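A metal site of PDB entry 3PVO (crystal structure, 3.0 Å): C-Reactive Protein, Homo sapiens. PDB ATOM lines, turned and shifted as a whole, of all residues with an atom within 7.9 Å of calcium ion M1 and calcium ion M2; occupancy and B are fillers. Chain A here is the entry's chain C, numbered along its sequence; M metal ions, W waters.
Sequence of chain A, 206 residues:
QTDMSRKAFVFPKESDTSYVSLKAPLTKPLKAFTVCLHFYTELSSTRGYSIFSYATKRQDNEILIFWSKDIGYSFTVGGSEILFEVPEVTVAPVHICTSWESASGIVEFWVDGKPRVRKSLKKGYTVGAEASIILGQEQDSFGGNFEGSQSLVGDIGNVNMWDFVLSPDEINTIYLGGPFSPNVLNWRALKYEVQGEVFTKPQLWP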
ATOM      1  N   SER A  50      22.406   2.286 -16.343  1.00  0.00           N
ATOM      2  CA  SER A  50      21.850   3.441 -17.016  1.00  0.00           C
ATOM      3  C   SER A  50      22.943   4.277 -17.684  1.00  0.00           C
ATOM      4  O   SER A  50      23.990   4.571 -17.101  1.00  0.00           O
ATOM      5  CB  SER A  50      21.020   4.276 -16.045  1.00  0.00           C
ATOM      6  OG  SER A  50      20.633   5.503 -16.646  1.00  0.00           O
ATOM      7  N   SER A  53      20.082   9.427 -18.200  1.00  0.00           N
ATOM      8  CA  SER A  53      18.822   9.566 -17.456  1.00  0.00           C
ATOM      9  C   SER A  53      18.269  10.961 -17.479  1.00  0.00           C
ATOM     10  O   SER A  53      18.875  11.887 -16.955  1.00  0.00           O
ATOM     11  CB  SER A  53      18.975   9.121 -16.010  1.00  0.00           C
ATOM     12  OG  SER A  53      17.733   9.187 -15.342  1.00  0.00           O
ATOM     13  N   ALA A  55      14.934  12.977 -16.422  1.00  0.00           N
ATOM     14  CA  ALA A  55      13.747  12.878 -15.585  1.00  0.00           C
ATOM     15  C   ALA A  55      12.978  14.191 -15.463  1.00  0.00           C
ATOM     16  O   ALA A  55      13.573  15.255 -15.473  1.00  0.00           O
ATOM     17  CB  ALA A  55      14.120  12.368 -14.205  1.00  0.00           C
ATOM     18  N   GLN A  59       7.514  12.216 -14.738  1.00  0.00           N
ATOM     19  CA  GLN A  59       7.983  10.944 -15.250  1.00  0.00           C
ATOM     20  C   GLN A  59       9.470  10.719 -14.987  1.00  0.00           C
ATOM     21  O   GLN A  59      10.328  11.435 -15.516  1.00  0.00           O
ATOM     22  CB  GLN A  59       7.689  10.846 -16.752  1.00  0.00           C
ATOM     23  CG  GLN A  59       8.225   9.596 -17.424  1.00  0.00           C
ATOM     24  CD  GLN A  59       7.701   8.323 -16.796  1.00  0.00           C
ATOM     25  OE1 GLN A  59       8.406   7.633 -16.077  1.00  0.00           O
ATOM     26  NE2 GLN A  59       6.471   8.002 -17.066  1.00  0.00           N
ATOM     27  N   ASP A  60       9.757   9.706 -14.167  1.00  0.00           N
ATOM     28  CA  ASP A  60      11.139   9.405 -13.773  1.00  0.00           C
ATOM     29  C   ASP A  60      12.009   8.896 -14.930  1.00  0.00           C
ATOM     30  O   ASP A  60      13.217   9.059 -14.926  1.00  0.00           O
ATOM     31  CB  ASP A  60      11.182   8.459 -12.562  1.00  0.00           C
ATOM     32  CG  ASP A  60      10.858   7.022 -12.926  1.00  0.00           C
ATOM     33  OD1 ASP A  60       9.756   6.748 -13.461  1.00  0.00           O
ATOM     34  OD2 ASP A  60      11.707   6.149 -12.648  1.00  0.00           O
ATOM     35  N   ASN A  61      11.371   8.272 -15.917  1.00  0.00           N
ATOM     36  CA  ASN A  61      12.049   7.831 -17.110  1.00  0.00           C
ATOM     37  C   ASN A  61      11.483   8.547 -18.303  1.00  0.00           C
ATOM     38  O   ASN A  61      10.879   7.909 -19.175  1.00  0.00           O
ATOM     39  CB  ASN A  61      11.877   6.321 -17.289  1.00  0.00           C
ATOM     40  CG  ASN A  61      12.417   5.529 -16.142  1.00  0.00           C
ATOM     41  OD1 ASN A  61      13.141   6.043 -15.276  1.00  0.00           O
ATOM     42  ND2 ASN A  61      12.065   4.251 -16.113  1.00  0.00           N
ATOM     43  N   GLU A  62      11.665   9.867 -18.353  1.00  0.00           N
ATOM     44  CA  GLU A  62      11.197  10.668 -19.487  1.00  0.00           C
ATOM     45  C   GLU A  62      11.962  10.380 -20.756  1.00  0.00           C
ATOM     46  O   GLU A  62      11.366  10.266 -21.818  1.00  0.00           O
ATOM     47  CB  GLU A  62      11.263  12.173 -19.177  1.00  0.00           C
ATOM     48  CG  GLU A  62      10.640  13.083 -20.239  1.00  0.00           C
ATOM     49  CD  GLU A  62       9.135  13.087 -20.204  1.00  0.00           C
ATOM     50  OE1 GLU A  62       8.518  11.994 -20.148  1.00  0.00           O
ATOM     51  OE2 GLU A  62       8.550  14.194 -20.224  1.00  0.00           O
ATOM     52  N   LEU A  64      15.207   7.597 -21.305  1.00  0.00           N
ATOM     53  CA  LEU A  64      16.176   6.728 -20.690  1.00  0.00           C
ATOM     54  C   LEU A  64      16.907   5.876 -21.720  1.00  0.00           C
ATOM     55  O   LEU A  64      16.287   5.115 -22.454  1.00  0.00           O
ATOM     56  CB  LEU A  64      15.486   5.859 -19.643  1.00  0.00           C
ATOM     57  CG  LEU A  64      16.377   4.939 -18.836  1.00  0.00           C
ATOM     58  CD1 LEU A  64      17.445   5.740 -18.098  1.00  0.00           C
ATOM     59  CD2 LEU A  64      15.488   4.201 -17.877  1.00  0.00           C
ATOM     60  N   PHE A  66      19.383   2.890 -21.558  1.00  0.00           N
ATOM     61  CA  PHE A  66      19.690   1.872 -20.558  1.00  0.00           C
ATOM     62  C   PHE A  66      20.290   0.668 -21.247  1.00  0.00           C
ATOM     63  O   PHE A  66      20.019   0.437 -22.423  1.00  0.00           O
ATOM     64  CB  PHE A  66      18.410   1.460 -19.817  1.00  0.00           C
ATOM     65  CG  PHE A  66      18.649   0.741 -18.524  1.00  0.00           C
ATOM     66  CD1 PHE A  66      18.742   1.401 -17.343  1.00  0.00           C
ATOM     67  CD2 PHE A  66      18.732  -0.605 -18.455  1.00  0.00           C
ATOM     68  CE1 PHE A  66      18.946   0.711 -16.128  1.00  0.00           C
ATOM     69  CE2 PHE A  66      18.935  -1.273 -17.247  1.00  0.00           C
ATOM     70  CZ  PHE A  66      19.044  -0.622 -16.098  1.00  0.00           C
ATOM     71  N   GLN A 137      23.921   7.317 -13.045  1.00  0.00           N
ATOM     72  CA  GLN A 137      22.866   6.783 -12.193  1.00  0.00           C
ATOM     73  C   GLN A 137      21.511   6.768 -12.876  1.00  0.00           C
ATOM     74  O   GLN A 137      21.237   7.556 -13.777  1.00  0.00           O
ATOM     75  CB  GLN A 137      22.711   7.611 -10.918  1.00  0.00           C
ATOM     76  CG  GLN A 137      23.940   7.709 -10.022  1.00  0.00           C
ATOM     77  CD  GLN A 137      24.429   6.361  -9.552  1.00  0.00           C
ATOM     78  OE1 GLN A 137      25.627   6.167  -9.380  1.00  0.00           O
ATOM     79  NE2 GLN A 137      23.507   5.426  -9.347  1.00  0.00           N
ATOM     80  N   GLU A 138      20.646   5.857 -12.434  1.00  0.00           N
ATOM     81  CA  GLU A 138      19.269   5.818 -12.913  1.00  0.00           C
ATOM     82  C   GLU A 138      18.308   6.457 -11.908  1.00  0.00           C
ATOM     83  O   GLU A 138      18.135   5.986 -10.761  1.00  0.00           O
ATOM     84  CB  GLU A 138      18.830   4.387 -13.213  1.00  0.00           C
ATOM     85  CG  GLU A 138      17.639   4.281 -14.147  1.00  0.00           C
ATOM     86  CD  GLU A 138      16.317   4.384 -13.443  1.00  0.00           C
ATOM     87  OE1 GLU A 138      16.143   3.707 -12.402  1.00  0.00           O
ATOM     88  OE2 GLU A 138      15.443   5.134 -13.933  1.00  0.00           O
ATOM     89  N   GLN A 139      17.673   7.535 -12.368  1.00  0.00           N
ATOM     90  CA  GLN A 139      16.659   8.258 -11.614  1.00  0.00           C
ATOM     91  C   GLN A 139      15.351   7.469 -11.431  1.00  0.00           C
ATOM     92  O   GLN A 139      14.798   6.881 -12.382  1.00  0.00           O
ATOM     93  CB  GLN A 139      16.403   9.608 -12.259  1.00  0.00           C
ATOM     94  CG  GLN A 139      17.591  10.553 -12.126  1.00  0.00           C
ATOM     95  CD  GLN A 139      17.492  11.814 -12.967  1.00  0.00           C
ATOM     96  OE1 GLN A 139      17.724  11.794 -14.172  1.00  0.00           O
ATOM     97  NE2 GLN A 139      17.199  12.924 -12.320  1.00  0.00           N
ATOM     98  N   ASP A 140      14.867   7.438 -10.190  1.00  0.00           N
ATOM     99  CA  ASP A 140      13.541   6.930  -9.879  1.00  0.00           C
ATOM    100  C   ASP A 140      12.706   8.066  -9.292  1.00  0.00           C
ATOM    101  O   ASP A 140      11.520   7.920  -9.028  1.00  0.00           O
ATOM    102  CB  ASP A 140      13.623   5.737  -8.918  1.00  0.00           C
ATOM    103  CG  ASP A 140      14.142   4.475  -9.582  1.00  0.00           C
ATOM    104  OD1 ASP A 140      14.106   4.329 -10.811  1.00  0.00           O
ATOM    105  OD2 ASP A 140      14.601   3.584  -8.878  1.00  0.00           O
ATOM    106  N   SER A 141      13.357   9.202  -9.090  1.00  0.00           N
ATOM    107  CA  SER A 141      12.682  10.448  -8.720  1.00  0.00           C
ATOM    108  C   SER A 141      13.457  11.641  -9.309  1.00  0.00           C
ATOM    109  O   SER A 141      14.616  11.505  -9.724  1.00  0.00           O
ATOM    110  CB  SER A 141      12.512  10.564  -7.184  1.00  0.00           C
ATOM    111  OG  SER A 141      13.734  10.865  -6.511  1.00  0.00           O
ATOM    112  N   GLY A 144      17.111  12.188  -8.093  1.00  0.00           N
ATOM    113  CA  GLY A 144      17.498  11.286  -7.008  1.00  0.00           C
ATOM    114  C   GLY A 144      16.988   9.867  -7.095  1.00  0.00           C
ATOM    115  O   GLY A 144      16.647   9.372  -8.162  1.00  0.00           O
ATOM    116  N   ASN A 145      16.972   9.206  -5.930  1.00  0.00           N
ATOM    117  CA  ASN A 145      16.557   7.801  -5.795  1.00  0.00           C
ATOM    118  C   ASN A 145      17.313   6.842  -6.690  1.00  0.00           C
ATOM    119  O   ASN A 145      16.729   6.067  -7.447  1.00  0.00           O
ATOM    120  CB  ASN A 145      15.047   7.652  -5.999  1.00  0.00           C
ATOM    121  CG  ASN A 145      14.269   7.994  -4.786  1.00  0.00           C
ATOM    122  OD1 ASN A 145      13.698   7.175  -4.175  1.00  0.00           O
ATOM    123  ND2 ASN A 145      14.237   9.207  -4.439  1.00  0.00           N
ATOM    124  N   PHE A 146      18.628   6.888  -6.574  1.00  0.00           N
ATOM    125  CA  PHE A 146      19.492   6.115  -7.442  1.00  0.00           C
ATOM    126  C   PHE A 146      19.565   4.696  -6.963  1.00  0.00           C
ATOM    127  O   PHE A 146      19.282   4.417  -5.802  1.00  0.00           O
ATOM    128  CB  PHE A 146      20.886   6.735  -7.461  1.00  0.00           C
ATOM    129  CG  PHE A 146      20.899   8.222  -7.766  1.00  0.00           C
ATOM    130  CD1 PHE A 146      20.218   8.722  -8.867  1.00  0.00           C
ATOM    131  CD2 PHE A 146      21.610   9.101  -6.960  1.00  0.00           C
ATOM    132  CE1 PHE A 146      20.250  10.080  -9.156  1.00  0.00           C
ATOM    133  CE2 PHE A 146      21.644  10.462  -7.240  1.00  0.00           C
ATOM    134  CZ  PHE A 146      20.965  10.941  -8.334  1.00  0.00           C
ATOM    135  N   GLU A 147      19.926   3.791  -7.859  1.00  0.00           N
ATOM    136  CA  GLU A 147      20.185   2.430  -7.468  1.00  0.00           C
ATOM    137  C   GLU A 147      21.577   2.035  -7.900  1.00  0.00           C
ATOM    138  O   GLU A 147      21.891   2.097  -9.073  1.00  0.00           O
ATOM    139  CB  GLU A 147      19.160   1.490  -8.073  1.00  0.00           C
ATOM    140  CG  GLU A 147      17.750   1.791  -7.607  1.00  0.00           C
ATOM    141  CD  GLU A 147      16.742   0.777  -8.086  1.00  0.00           C
ATOM    142  OE1 GLU A 147      16.716  -0.328  -7.601  1.00  0.00           O
ATOM    143  OE2 GLU A 147      15.948   1.028  -8.978  1.00  0.00           O
ATOM    144  N   GLY A 148      22.390   1.622  -6.929  1.00  0.00           N
ATOM    145  CA  GLY A 148      23.740   1.143  -7.209  1.00  0.00           C
ATOM    146  C   GLY A 148      23.824   0.033  -8.251  1.00  0.00           C
ATOM    147  O   GLY A 148      24.774  -0.033  -9.030  1.00  0.00           O
ATOM    148  N   SER A 149      22.818  -0.844  -8.250  1.00  0.00           N
ATOM    149  CA  SER A 149      22.757  -1.942  -9.213  1.00  0.00           C
ATOM    150  C   SER A 149      22.422  -1.465 -10.633  1.00  0.00           C
ATOM    151  O   SER A 149      22.477  -2.239 -11.595  1.00  0.00           O
ATOM    152  CB  SER A 149      21.791  -3.031  -8.747  1.00  0.00           C
ATOM    153  OG  SER A 149      20.497  -2.515  -8.543  1.00  0.00           O
ATOM    154  N   GLN A 150      22.123  -0.176 -10.759  1.00  0.00           N
ATOM    155  CA  GLN A 150      21.876   0.453 -12.052  1.00  0.00           C
ATOM    156  C   GLN A 150      22.883   1.562 -12.341  1.00  0.00           C
ATOM    157  O   GLN A 150      22.621   2.417 -13.180  1.00  0.00           O
ATOM    158  CB  GLN A 150      20.446   0.996 -12.129  1.00  0.00           C
ATOM    159  CG  GLN A 150      19.360  -0.059 -11.906  1.00  0.00           C
ATOM    160  CD  GLN A 150      17.967   0.481 -12.096  1.00  0.00           C
ATOM    161  OE1 GLN A 150      17.540   1.419 -11.443  1.00  0.00           O
ATOM    162  NE2 GLN A 150      17.212  -0.146 -12.984  1.00  0.00           N
HETATM  163 CA    CA M   1      16.037   2.841 -10.577  1.00  0.00          CA
HETATM  164 CA    CA M   2      13.540   5.177 -13.083  1.00  0.00          CA
HETATM  165  O   HOH W   1      14.035   1.978 -13.126  1.00  0.00           O
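The side-chain carboxylate (OD1) of Asp 60 sits close to the side-chain amide oxygen (OE1) of Gln 59 (3.1 Å). N of Ser 50 sits at hydrogen-bond distance from O of Gln 150 (3.2 Å). OG of Ser 53 lies within hydrogen-bond range of OE1 of Gln 139 (2.9 Å). The side-chain amide oxygen of Gln 59 lies within hydrogen-bond range of the backbone NH of Asn 61, at 3.0 Å.
Along chain A the residues within 4 Å of calcium ion M2 span positions 60 to 140.
Calcium ion M1 is bound by OE1 of Glu 138, OE1 of Gln 150, OD2 of Asp 140, OE2 of Glu 147 and OD1 of Asp 140. Calcium ion M1 has five donor atoms within binding distance.
Calcium ion M2 is bound by the side-chain carboxylate (OE2) of Glu 138 (2.1 Å), the side-chain carboxylate (OD2) of Asp 60 (2.1 Å), the backbone carbonyl oxygen (O) of Gln 139 (2.2 Å), the side-chain amide oxygen (OD1) of Asn 61 (2.4 Å) and the side-chain carboxylate (OD1) of Asp 140 (2.5 Å). Slightly farther from calcium ion M2 lies the side-chain carboxylate (OE1) of Glu 138 (3.1 Å).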
